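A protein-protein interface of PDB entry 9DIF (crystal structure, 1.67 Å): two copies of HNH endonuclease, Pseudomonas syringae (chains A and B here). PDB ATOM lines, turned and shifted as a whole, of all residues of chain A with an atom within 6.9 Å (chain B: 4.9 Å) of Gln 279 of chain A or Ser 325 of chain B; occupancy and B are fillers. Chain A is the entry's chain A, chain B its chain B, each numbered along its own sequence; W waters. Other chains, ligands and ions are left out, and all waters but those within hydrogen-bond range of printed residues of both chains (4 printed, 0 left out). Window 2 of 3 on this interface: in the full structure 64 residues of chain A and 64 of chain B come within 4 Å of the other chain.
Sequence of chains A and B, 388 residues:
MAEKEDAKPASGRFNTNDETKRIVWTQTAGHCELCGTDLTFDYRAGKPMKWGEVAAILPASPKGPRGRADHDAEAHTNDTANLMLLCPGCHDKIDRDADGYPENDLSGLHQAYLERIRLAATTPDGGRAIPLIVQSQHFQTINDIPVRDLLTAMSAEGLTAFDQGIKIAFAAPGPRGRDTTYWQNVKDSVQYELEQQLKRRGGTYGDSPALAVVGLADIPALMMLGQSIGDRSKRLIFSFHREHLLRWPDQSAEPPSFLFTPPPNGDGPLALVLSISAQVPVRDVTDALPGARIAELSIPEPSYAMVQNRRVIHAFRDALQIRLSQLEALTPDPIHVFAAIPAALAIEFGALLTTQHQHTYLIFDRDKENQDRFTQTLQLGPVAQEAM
The backbone carbonyl oxygen (O) of Ser 277 of chain A is in hydrogen-bond range of the side-chain amide nitrogen (NE2) of Gln 321 of chain B.
The backbone NH (N) of Tyr 304 of chain A sits at hydrogen-bond distance from the side-chain amide oxygen (OE1) of Gln 321 of chain B (3.0 Å).
The side-chain hydroxyl of Ser 325 of chain B is in hydrogen-bond range of the backbone NH of Gln 279 of chain A (3.0 Å).
The backbone carbonyl oxygen (O) of Ile 276 of chain A is in hydrogen-bond range of the backbone NH (N) of Ser 303 of chain A (3.1 Å).
The backbone NH (N) of Ser 303 of chain A lies within hydrogen-bond range of the backbone carbonyl oxygen (O) of Ser 277 of chain A (3.4 Å).
The side-chain hydroxyl (OG) of Ser 275 of chain A sits at hydrogen-bond distance from the side-chain amide nitrogen (NE2) of Gln 279 of chain A (3.5 Å).
The side-chain amide nitrogen (NE2) of Gln 279 of chain A sits at hydrogen-bond distance from the side-chain carboxylate (OE2) of Glu 296 of chain A (3.2 Å).
The backbone carbonyl oxygen (O) of Ala 340 of chain A is in hydrogen-bond range of the backbone NH (N) of Ser 277 of chain A.
OE1 of Gln 326 of chain B sits close to O of Ile 322 of chain B (3.4 Å).
CA of Ala 278 of chain A touches OG of Ser 325 of chain B (3.5 Å).
Glu 301 of chain A touches Ile 322 of chain B (OE1 to CD1, 3.6 Å).
Ile 322 of chain B touches Pro 302 of chain A.
Gln 321 of chain B touches Ser 303 of chain A (OE1 to CA, 3.3 Å).
Ser 303 of chain A touches Ile 322 of chain B (CB to CG1, 3.8 Å).
Printed residues of chain B within 4 Å of Gln 279 of chain A: Ser 325 (3.0 Å).
Ser 325 of chain B touches just these residues of chain A: Ala 278 (3.5 Å) and Gln 279 (3.0 Å).
Of the printed residues of chain B, Ser 277 of chain A touches Gln 321.
Of the printed residues of chain B, Ser 303 of chain A touches Gln 321 (3.3 Å) and Ile 322 (3.8 Å).
Arg 323 of chain B touches none of the printed residues of chain A.
Ile 299 of chain A touches none of the printed residues of chain B.
Printed residues of chain A that touch a printed residue of chain B: Ser 277, Ala 278, Gln 279, Glu 301, Pro 302, Ser 303 and Tyr 304.
Hydrophobic or aromatic side chains of chain A within 4 Å of the printed part of chain B: Ala 278 and Tyr 304.
Hydrophobic or aromatic side chains of chain B within 4 Å of the printed part of chain A: Ile 322.
No position is printed for both chains.
Water W3 bridges OE2 of Glu 301 of chain A (2.5 Å) and OE1 of Gln 326 of chain B (3.4 Å).
Water W4 lies within hydrogen-bond range of OE1 of Gln 321 of chain B (2.6 Å) and OG of Ser 303 of chain A (2.7 Å).
Water W2 lies within hydrogen-bond range of O of Gln 279 of chain A and O of Ser 325 of chain B.
Water W1 bridges O of Pro 302 of chain A (2.8 Å) and O of Ile 322 of chain B (2.9 Å).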
ATOM      1  N   VAL A 273      17.137  15.177  -2.504  1.00  0.00           N
ATOM      2  CA  VAL A 273      18.496  14.822  -2.874  1.00  0.00           C
ATOM      3  C   VAL A 273      19.481  15.894  -2.404  1.00  0.00           C
ATOM      4  O   VAL A 273      19.335  17.087  -2.724  1.00  0.00           O
ATOM      5  CB  VAL A 273      18.579  14.601  -4.390  1.00  0.00           C
ATOM      6  CG1 VAL A 273      19.992  14.211  -4.807  1.00  0.00           C
ATOM      7  CG2 VAL A 273      17.635  13.488  -4.832  1.00  0.00           C
ATOM      8  N   LEU A 274      20.541  15.465  -1.740  1.00  0.00           N
ATOM      9  CA  LEU A 274      21.561  16.365  -1.209  1.00  0.00           C
ATOM     10  C   LEU A 274      22.847  16.010  -1.930  1.00  0.00           C
ATOM     11  O   LEU A 274      23.412  14.937  -1.682  1.00  0.00           O
ATOM     12  CB  LEU A 274      21.722  16.251   0.305  1.00  0.00           C
ATOM     13  CG  LEU A 274      20.442  16.382   1.160  1.00  0.00           C
ATOM     14  CD1 LEU A 274      20.710  16.181   2.656  1.00  0.00           C
ATOM     15  CD2 LEU A 274      19.741  17.711   0.960  1.00  0.00           C
ATOM     16  N   SER A 275      23.311  16.902  -2.804  1.00  0.00           N
ATOM     17  CA  SER A 275      24.508  16.699  -3.621  1.00  0.00           C
ATOM     18  C   SER A 275      25.608  17.667  -3.191  1.00  0.00           C
ATOM     19  O   SER A 275      25.816  18.694  -3.818  1.00  0.00           O
ATOM     20  CB  SER A 275      24.175  16.886  -5.079  1.00  0.00           C
ATOM     21  OG  SER A 275      23.465  15.770  -5.600  1.00  0.00           O
ATOM     22  N   ILE A 276      26.321  17.345  -2.112  1.00  0.00           N
ATOM     23  CA  ILE A 276      27.236  18.277  -1.471  1.00  0.00           C
ATOM     24  C   ILE A 276      28.651  17.730  -1.514  1.00  0.00           C
ATOM     25  O   ILE A 276      29.571  18.382  -2.012  1.00  0.00           O
ATOM     26  CB  ILE A 276      26.819  18.563   0.002  1.00  0.00           C
ATOM     27  CG1 ILE A 276      25.401  19.120   0.159  1.00  0.00           C
ATOM     28  CG2 ILE A 276      27.777  19.548   0.671  1.00  0.00           C
ATOM     29  CD1 ILE A 276      25.160  20.426  -0.514  1.00  0.00           C
ATOM     30  N   SER A 277      28.822  16.472  -1.083  1.00  0.00           N
ATOM     31  CA  SER A 277      30.068  15.717  -1.237  1.00  0.00           C
ATOM     32  C   SER A 277      30.303  15.310  -2.677  1.00  0.00           C
ATOM     33  O   SER A 277      31.450  15.234  -3.120  1.00  0.00           O
ATOM     34  CB  SER A 277      30.077  14.444  -0.400  1.00  0.00           C
ATOM     35  OG  SER A 277      29.988  14.784   0.950  1.00  0.00           O
ATOM     36  N   ALA A 278      29.236  15.092  -3.436  1.00  0.00           N
ATOM     37  CA  ALA A 278      29.290  14.502  -4.773  1.00  0.00           C
ATOM     38  C   ALA A 278      27.913  14.735  -5.398  1.00  0.00           C
ATOM     39  O   ALA A 278      26.927  14.983  -4.692  1.00  0.00           O
ATOM     40  CB  ALA A 278      29.636  12.997  -4.762  1.00  0.00           C
ATOM     41  N   GLN A 279      27.864  14.664  -6.727  1.00  0.00           N
ATOM     42  CA  GLN A 279      26.610  14.705  -7.473  1.00  0.00           C
ATOM     43  C   GLN A 279      25.945  13.336  -7.418  1.00  0.00           C
ATOM     44  O   GLN A 279      26.500  12.354  -7.922  1.00  0.00           O
ATOM     45  CB  GLN A 279      26.866  15.094  -8.925  1.00  0.00           C
ATOM     46  CG  GLN A 279      25.564  15.197  -9.761  1.00  0.00           C
ATOM     47  CD  GLN A 279      24.569  16.177  -9.219  1.00  0.00           C
ATOM     48  OE1 GLN A 279      24.904  17.330  -8.944  1.00  0.00           O
ATOM     49  NE2 GLN A 279      23.327  15.722  -9.054  1.00  0.00           N
ATOM     50  N   VAL A 280      24.766  13.276  -6.795  1.00  0.00           N
ATOM     51  CA  VAL A 280      23.930  12.078  -6.813  1.00  0.00           C
ATOM     52  C   VAL A 280      23.289  11.953  -8.195  1.00  0.00           C
ATOM     53  O   VAL A 280      22.593  12.872  -8.636  1.00  0.00           O
ATOM     54  CB  VAL A 280      22.867  12.128  -5.698  1.00  0.00           C
ATOM     55  CG1 VAL A 280      21.954  10.914  -5.748  1.00  0.00           C
ATOM     56  CG2 VAL A 280      23.543  12.218  -4.305  1.00  0.00           C
ATOM     57  N   PRO A 281      23.493  10.840  -8.915  1.00  0.00           N
ATOM     58  CA  PRO A 281      22.841  10.684 -10.223  1.00  0.00           C
ATOM     59  C   PRO A 281      21.331  10.469 -10.067  1.00  0.00           C
ATOM     60  O   PRO A 281      20.875   9.643  -9.279  1.00  0.00           O
ATOM     61  CB  PRO A 281      23.550   9.454 -10.830  1.00  0.00           C
ATOM     62  CG  PRO A 281      24.753   9.258 -10.060  1.00  0.00           C
ATOM     63  CD  PRO A 281      24.431   9.739  -8.663  1.00  0.00           C
ATOM     64  N   VAL A 282      20.547  11.177 -10.882  1.00  0.00           N
ATOM     65  CA  VAL A 282      19.090  11.003 -10.818  1.00  0.00           C
ATOM     66  C   VAL A 282      18.689   9.555 -11.090  1.00  0.00           C
ATOM     67  O   VAL A 282      17.761   9.019 -10.457  1.00  0.00           O
ATOM     68  CB  VAL A 282      18.397  11.986 -11.786  1.00  0.00           C
ATOM     69  CG1 VAL A 282      18.611  13.422 -11.300  1.00  0.00           C
ATOM     70  CG2 VAL A 282      18.930  11.851 -13.142  1.00  0.00           C
ATOM     71  N   GLU A 296      16.315  19.159  -4.946  1.00  0.00           N
ATOM     72  CA  GLU A 296      17.747  18.987  -4.725  1.00  0.00           C
ATOM     73  C   GLU A 296      18.412  20.219  -4.126  1.00  0.00           C
ATOM     74  O   GLU A 296      18.213  21.337  -4.603  1.00  0.00           O
ATOM     75  CB  GLU A 296      18.431  18.603  -6.049  1.00  0.00           C
ATOM     76  CG  GLU A 296      19.948  18.481  -5.924  1.00  0.00           C
ATOM     77  CD  GLU A 296      20.609  17.870  -7.131  1.00  0.00           C
ATOM     78  OE1 GLU A 296      20.586  18.499  -8.209  1.00  0.00           O
ATOM     79  OE2 GLU A 296      21.145  16.751  -6.996  1.00  0.00           O
ATOM     80  N   SER A 298      22.297  21.568  -3.441  1.00  0.00           N
ATOM     81  CA  SER A 298      23.630  21.255  -3.951  1.00  0.00           C
ATOM     82  C   SER A 298      24.541  22.468  -3.776  1.00  0.00           C
ATOM     83  O   SER A 298      24.114  23.538  -3.346  1.00  0.00           O
ATOM     84  CB  SER A 298      23.525  20.838  -5.413  1.00  0.00           C
ATOM     85  OG  SER A 298      23.371  21.991  -6.228  1.00  0.00           O
ATOM     86  N   ILE A 299      25.830  22.262  -4.040  1.00  0.00           N
ATOM     87  CA  ILE A 299      26.767  23.383  -4.144  1.00  0.00           C
ATOM     88  C   ILE A 299      27.333  23.383  -5.553  1.00  0.00           C
ATOM     89  O   ILE A 299      27.334  22.340  -6.238  1.00  0.00           O
ATOM     90  CB  ILE A 299      27.883  23.307  -3.086  1.00  0.00           C
ATOM     91  CG1 ILE A 299      28.627  21.990  -3.226  1.00  0.00           C
ATOM     92  CG2 ILE A 299      27.287  23.492  -1.679  1.00  0.00           C
ATOM     93  CD1 ILE A 299      29.934  21.921  -2.405  1.00  0.00           C
ATOM     94  N   GLU A 301      30.272  23.183  -6.804  1.00  0.00           N
ATOM     95  CA  GLU A 301      31.335  22.227  -7.062  1.00  0.00           C
ATOM     96  C   GLU A 301      31.381  21.181  -5.960  1.00  0.00           C
ATOM     97  O   GLU A 301      32.175  21.304  -5.018  1.00  0.00           O
ATOM     98  CB  GLU A 301      32.679  22.943  -7.176  1.00  0.00           C
ATOM     99  CG  GLU A 301      33.884  22.005  -7.539  1.00  0.00           C
ATOM    100  CD  GLU A 301      35.104  22.797  -8.001  1.00  0.00           C
ATOM    101  OE1 GLU A 301      35.773  23.390  -7.109  1.00  0.00           O
ATOM    102  OE2 GLU A 301      35.353  22.867  -9.237  1.00  0.00           O
ATOM    103  N   PRO A 302      30.554  20.128  -6.047  1.00  0.00           N
ATOM    104  CA  PRO A 302      30.558  19.088  -4.992  1.00  0.00           C
ATOM    105  C   PRO A 302      31.971  18.571  -4.719  1.00  0.00           C
ATOM    106  O   PRO A 302      32.728  18.272  -5.639  1.00  0.00           O
ATOM    107  CB  PRO A 302      29.653  17.998  -5.574  1.00  0.00           C
ATOM    108  CG  PRO A 302      28.637  18.804  -6.433  1.00  0.00           C
ATOM    109  CD  PRO A 302      29.513  19.887  -7.071  1.00  0.00           C
ATOM    110  N   SER A 303      32.321  18.458  -3.439  1.00  0.00           N
ATOM    111  CA  SER A 303      33.651  18.048  -3.046  1.00  0.00           C
ATOM    112  C   SER A 303      33.637  17.515  -1.621  1.00  0.00           C
ATOM    113  O   SER A 303      33.024  18.102  -0.715  1.00  0.00           O
ATOM    114  CB  SER A 303      34.612  19.227  -3.199  1.00  0.00           C
ATOM    115  OG  SER A 303      35.866  18.965  -2.588  1.00  0.00           O
ATOM    116  N   TYR A 304      34.393  16.445  -1.432  1.00  0.00           N
ATOM    117  CA  TYR A 304      34.547  15.852  -0.116  1.00  0.00           C
ATOM    118  C   TYR A 304      35.196  16.791   0.884  1.00  0.00           C
ATOM    119  O   TYR A 304      35.069  16.544   2.095  1.00  0.00           O
ATOM    120  CB  TYR A 304      35.452  14.622  -0.208  1.00  0.00           C
ATOM    121  CG  TYR A 304      34.888  13.325  -0.750  1.00  0.00           C
ATOM    122  CD1 TYR A 304      33.600  13.271  -1.248  1.00  0.00           C
ATOM    123  CD2 TYR A 304      35.678  12.132  -0.810  1.00  0.00           C
ATOM    124  CE1 TYR A 304      33.065  12.090  -1.748  1.00  0.00           C
ATOM    125  CE2 TYR A 304      35.144  10.938  -1.325  1.00  0.00           C
ATOM    126  CZ  TYR A 304      33.835  10.966  -1.805  1.00  0.00           C
ATOM    127  OH  TYR A 304      33.193   9.847  -2.256  1.00  0.00           O
ATOM    128  N   ALA A 340      24.552  12.586  -0.445  1.00  0.00           N
ATOM    129  CA  ALA A 340      26.005  12.434  -0.528  1.00  0.00           C
ATOM    130  C   ALA A 340      26.540  13.701   0.139  1.00  0.00           C
ATOM    131  O   ALA A 340      26.640  14.742  -0.510  1.00  0.00           O
ATOM    132  CB  ALA A 340      26.532  12.269  -1.970  1.00  0.00           C
ATOM    133  N   ARG A 366      23.445   4.027   0.115  1.00  0.00           N
ATOM    134  CA  ARG A 366      24.099   3.115  -0.809  1.00  0.00           C
ATOM    135  C   ARG A 366      24.242   1.767  -0.137  1.00  0.00           C
ATOM    136  O   ARG A 366      24.655   1.692   1.022  1.00  0.00           O
ATOM    137  CB  ARG A 366      25.479   3.608  -1.237  1.00  0.00           C
ATOM    138  CG  ARG A 366      25.425   4.889  -2.072  1.00  0.00           C
ATOM    139  CD  ARG A 366      24.721   4.632  -3.437  1.00  0.00           C
ATOM    140  NE  ARG A 366      24.965   5.765  -4.338  1.00  0.00           N
ATOM    141  CZ  ARG A 366      24.634   5.809  -5.618  1.00  0.00           C
ATOM    142  NH1 ARG A 366      24.095   4.759  -6.225  1.00  0.00           N
ATOM    143  NH2 ARG A 366      24.878   6.926  -6.316  1.00  0.00           N
ATOM    144  N   GLN B 321      38.776  14.001  -6.943  1.00  0.00           N
ATOM    145  CA  GLN B 321      37.438  13.623  -6.514  1.00  0.00           C
ATOM    146  C   GLN B 321      36.404  14.571  -7.078  1.00  0.00           C
ATOM    147  O   GLN B 321      35.324  14.138  -7.477  1.00  0.00           O
ATOM    148  CB  GLN B 321      37.383  13.580  -4.993  1.00  0.00           C
ATOM    149  CG  GLN B 321      36.038  13.098  -4.457  1.00  0.00           C
ATOM    150  CD  GLN B 321      35.001  14.242  -4.326  1.00  0.00           C
ATOM    151  OE1 GLN B 321      35.337  15.415  -4.032  1.00  0.00           O
ATOM    152  NE2 GLN B 321      33.738  13.888  -4.586  1.00  0.00           N
ATOM    153  N   ILE B 322      36.744  15.850  -7.229  1.00  0.00           N
ATOM    154  CA  ILE B 322      35.813  16.783  -7.868  1.00  0.00           C
ATOM    155  C   ILE B 322      35.449  16.304  -9.270  1.00  0.00           C
ATOM    156  O   ILE B 322      34.301  16.457  -9.720  1.00  0.00           O
ATOM    157  CB  ILE B 322      36.432  18.191  -7.908  1.00  0.00           C
ATOM    158  CG1 ILE B 322      36.253  18.890  -6.558  1.00  0.00           C
ATOM    159  CG2 ILE B 322      35.758  19.120  -8.970  1.00  0.00           C
ATOM    160  CD1 ILE B 322      37.184  20.112  -6.373  1.00  0.00           C
ATOM    161  N   ARG B 323      36.433  15.843 -10.022  1.00  0.00           N
ATOM    162  CA  ARG B 323      36.168  15.372 -11.381  1.00  0.00           C
ATOM    163  C   ARG B 323      35.534  13.975 -11.399  1.00  0.00           C
ATOM    164  O   ARG B 323      34.788  13.652 -12.337  1.00  0.00           O
ATOM    165  CB  ARG B 323      37.466  15.375 -12.210  1.00  0.00           C
ATOM    166  CG  ARG B 323      38.188  16.708 -12.235  1.00  0.00           C
ATOM    167  CD  ARG B 323      37.268  17.800 -12.692  1.00  0.00           C
ATOM    168  NE  ARG B 323      37.929  19.089 -12.828  1.00  0.00           N
ATOM    169  CZ  ARG B 323      37.340  20.152 -13.346  1.00  0.00           C
ATOM    170  NH1 ARG B 323      36.096  20.098 -13.782  1.00  0.00           N
ATOM    171  NH2 ARG B 323      38.000  21.308 -13.384  1.00  0.00           N
ATOM    172  N   LEU B 324      35.898  13.082 -10.474  1.00  0.00           N
ATOM    173  CA  LEU B 324      35.238  11.778 -10.467  1.00  0.00           C
ATOM    174  C   LEU B 324      33.749  11.920 -10.148  1.00  0.00           C
ATOM    175  O   LEU B 324      32.924  11.166 -10.685  1.00  0.00           O
ATOM    176  CB  LEU B 324      35.893  10.848  -9.458  1.00  0.00           C
ATOM    177  CG  LEU B 324      37.348  10.500  -9.664  1.00  0.00           C
ATOM    178  CD1 LEU B 324      37.718   9.413  -8.548  1.00  0.00           C
ATOM    179  CD2 LEU B 324      37.575   9.975 -11.040  1.00  0.00           C
ATOM    180  N   SER B 325      33.381  12.918  -9.345  1.00  0.00           N
ATOM    181  CA  SER B 325      31.964  13.159  -9.065  1.00  0.00           C
ATOM    182  C   SER B 325      31.224  13.531 -10.338  1.00  0.00           C
ATOM    183  O   SER B 325      30.163  12.956 -10.629  1.00  0.00           O
ATOM    184  CB  SER B 325      31.822  14.241  -8.006  1.00  0.00           C
ATOM    185  OG  SER B 325      30.518  14.737  -8.059  1.00  0.00           O
ATOM    186  N   GLN B 326      31.856  14.353 -11.186  1.00  0.00           N
ATOM    187  CA  GLN B 326      31.314  14.663 -12.508  1.00  0.00           C
ATOM    188  C   GLN B 326      31.235  13.436 -13.420  1.00  0.00           C
ATOM    189  O   GLN B 326      30.200  13.190 -14.047  1.00  0.00           O
ATOM    190  CB  GLN B 326      32.132  15.772 -13.169  1.00  0.00           C
ATOM    191  CG  GLN B 326      32.180  17.015 -12.373  1.00  0.00           C
ATOM    192  CD  GLN B 326      33.198  18.068 -12.925  1.00  0.00           C
ATOM    193  OE1 GLN B 326      33.884  18.744 -12.183  1.00  0.00           O
ATOM    194  NE2 GLN B 326      33.268  18.194 -14.210  1.00  0.00           N
ATOM    195  N   LEU B 327      32.333  12.679 -13.553  1.00  0.00           N
ATOM    196  CA  LEU B 327      32.362  11.536 -14.454  1.00  0.00           C
ATOM    197  C   LEU B 327      31.430  10.416 -14.002  1.00  0.00           C
ATOM    198  O   LEU B 327      30.716   9.843 -14.824  1.00  0.00           O
ATOM    199  CB  LEU B 327      33.787  11.022 -14.565  1.00  0.00           C
ATOM    200  CG  LEU B 327      34.768  12.002 -15.200  1.00  0.00           C
ATOM    201  CD1 LEU B 327      36.150  11.437 -15.127  1.00  0.00           C
ATOM    202  CD2 LEU B 327      34.453  12.298 -16.639  1.00  0.00           C
ATOM    203  N   GLU B 328      31.455  10.038 -12.713  1.00  0.00           N
ATOM    204  CA  GLU B 328      30.529   8.984 -12.261  1.00  0.00           C
ATOM    205  C   GLU B 328      29.052   9.358 -12.497  1.00  0.00           C
ATOM    206  O   GLU B 328      28.203   8.479 -12.747  1.00  0.00           O
ATOM    207  CB  GLU B 328      30.746   8.664 -10.775  1.00  0.00           C
ATOM    208  CG  GLU B 328      32.104   8.091 -10.432  1.00  0.00           C
ATOM    209  CD  GLU B 328      32.249   7.734  -8.939  1.00  0.00           C
ATOM    210  OE1 GLU B 328      31.265   7.849  -8.157  1.00  0.00           O
ATOM    211  OE2 GLU B 328      33.362   7.307  -8.538  1.00  0.00           O
ATOM    212  N   ALA B 329      28.717  10.647 -12.428  1.00  0.00           N
ATOM    213  CA  ALA B 329      27.357  11.080 -12.739  1.00  0.00           C
ATOM    214  C   ALA B 329      27.026  10.932 -14.219  1.00  0.00           C
ATOM    215  O   ALA B 329      25.844  10.796 -14.578  1.00  0.00           O
ATOM    216  CB  ALA B 329      27.166  12.532 -12.297  1.00  0.00           C
HETATM  217  O   HOH W   1      32.378  18.142  -8.416  1.00  0.00           O
HETATM  218  O   HOH W   2      28.808  11.465  -8.853  1.00  0.00           O
HETATM  219  O   HOH W   3      33.925  21.980 -11.143  1.00  0.00           O
HETATM  220  O   HOH W   4      37.330  16.998  -3.665  1.00  0.00           O
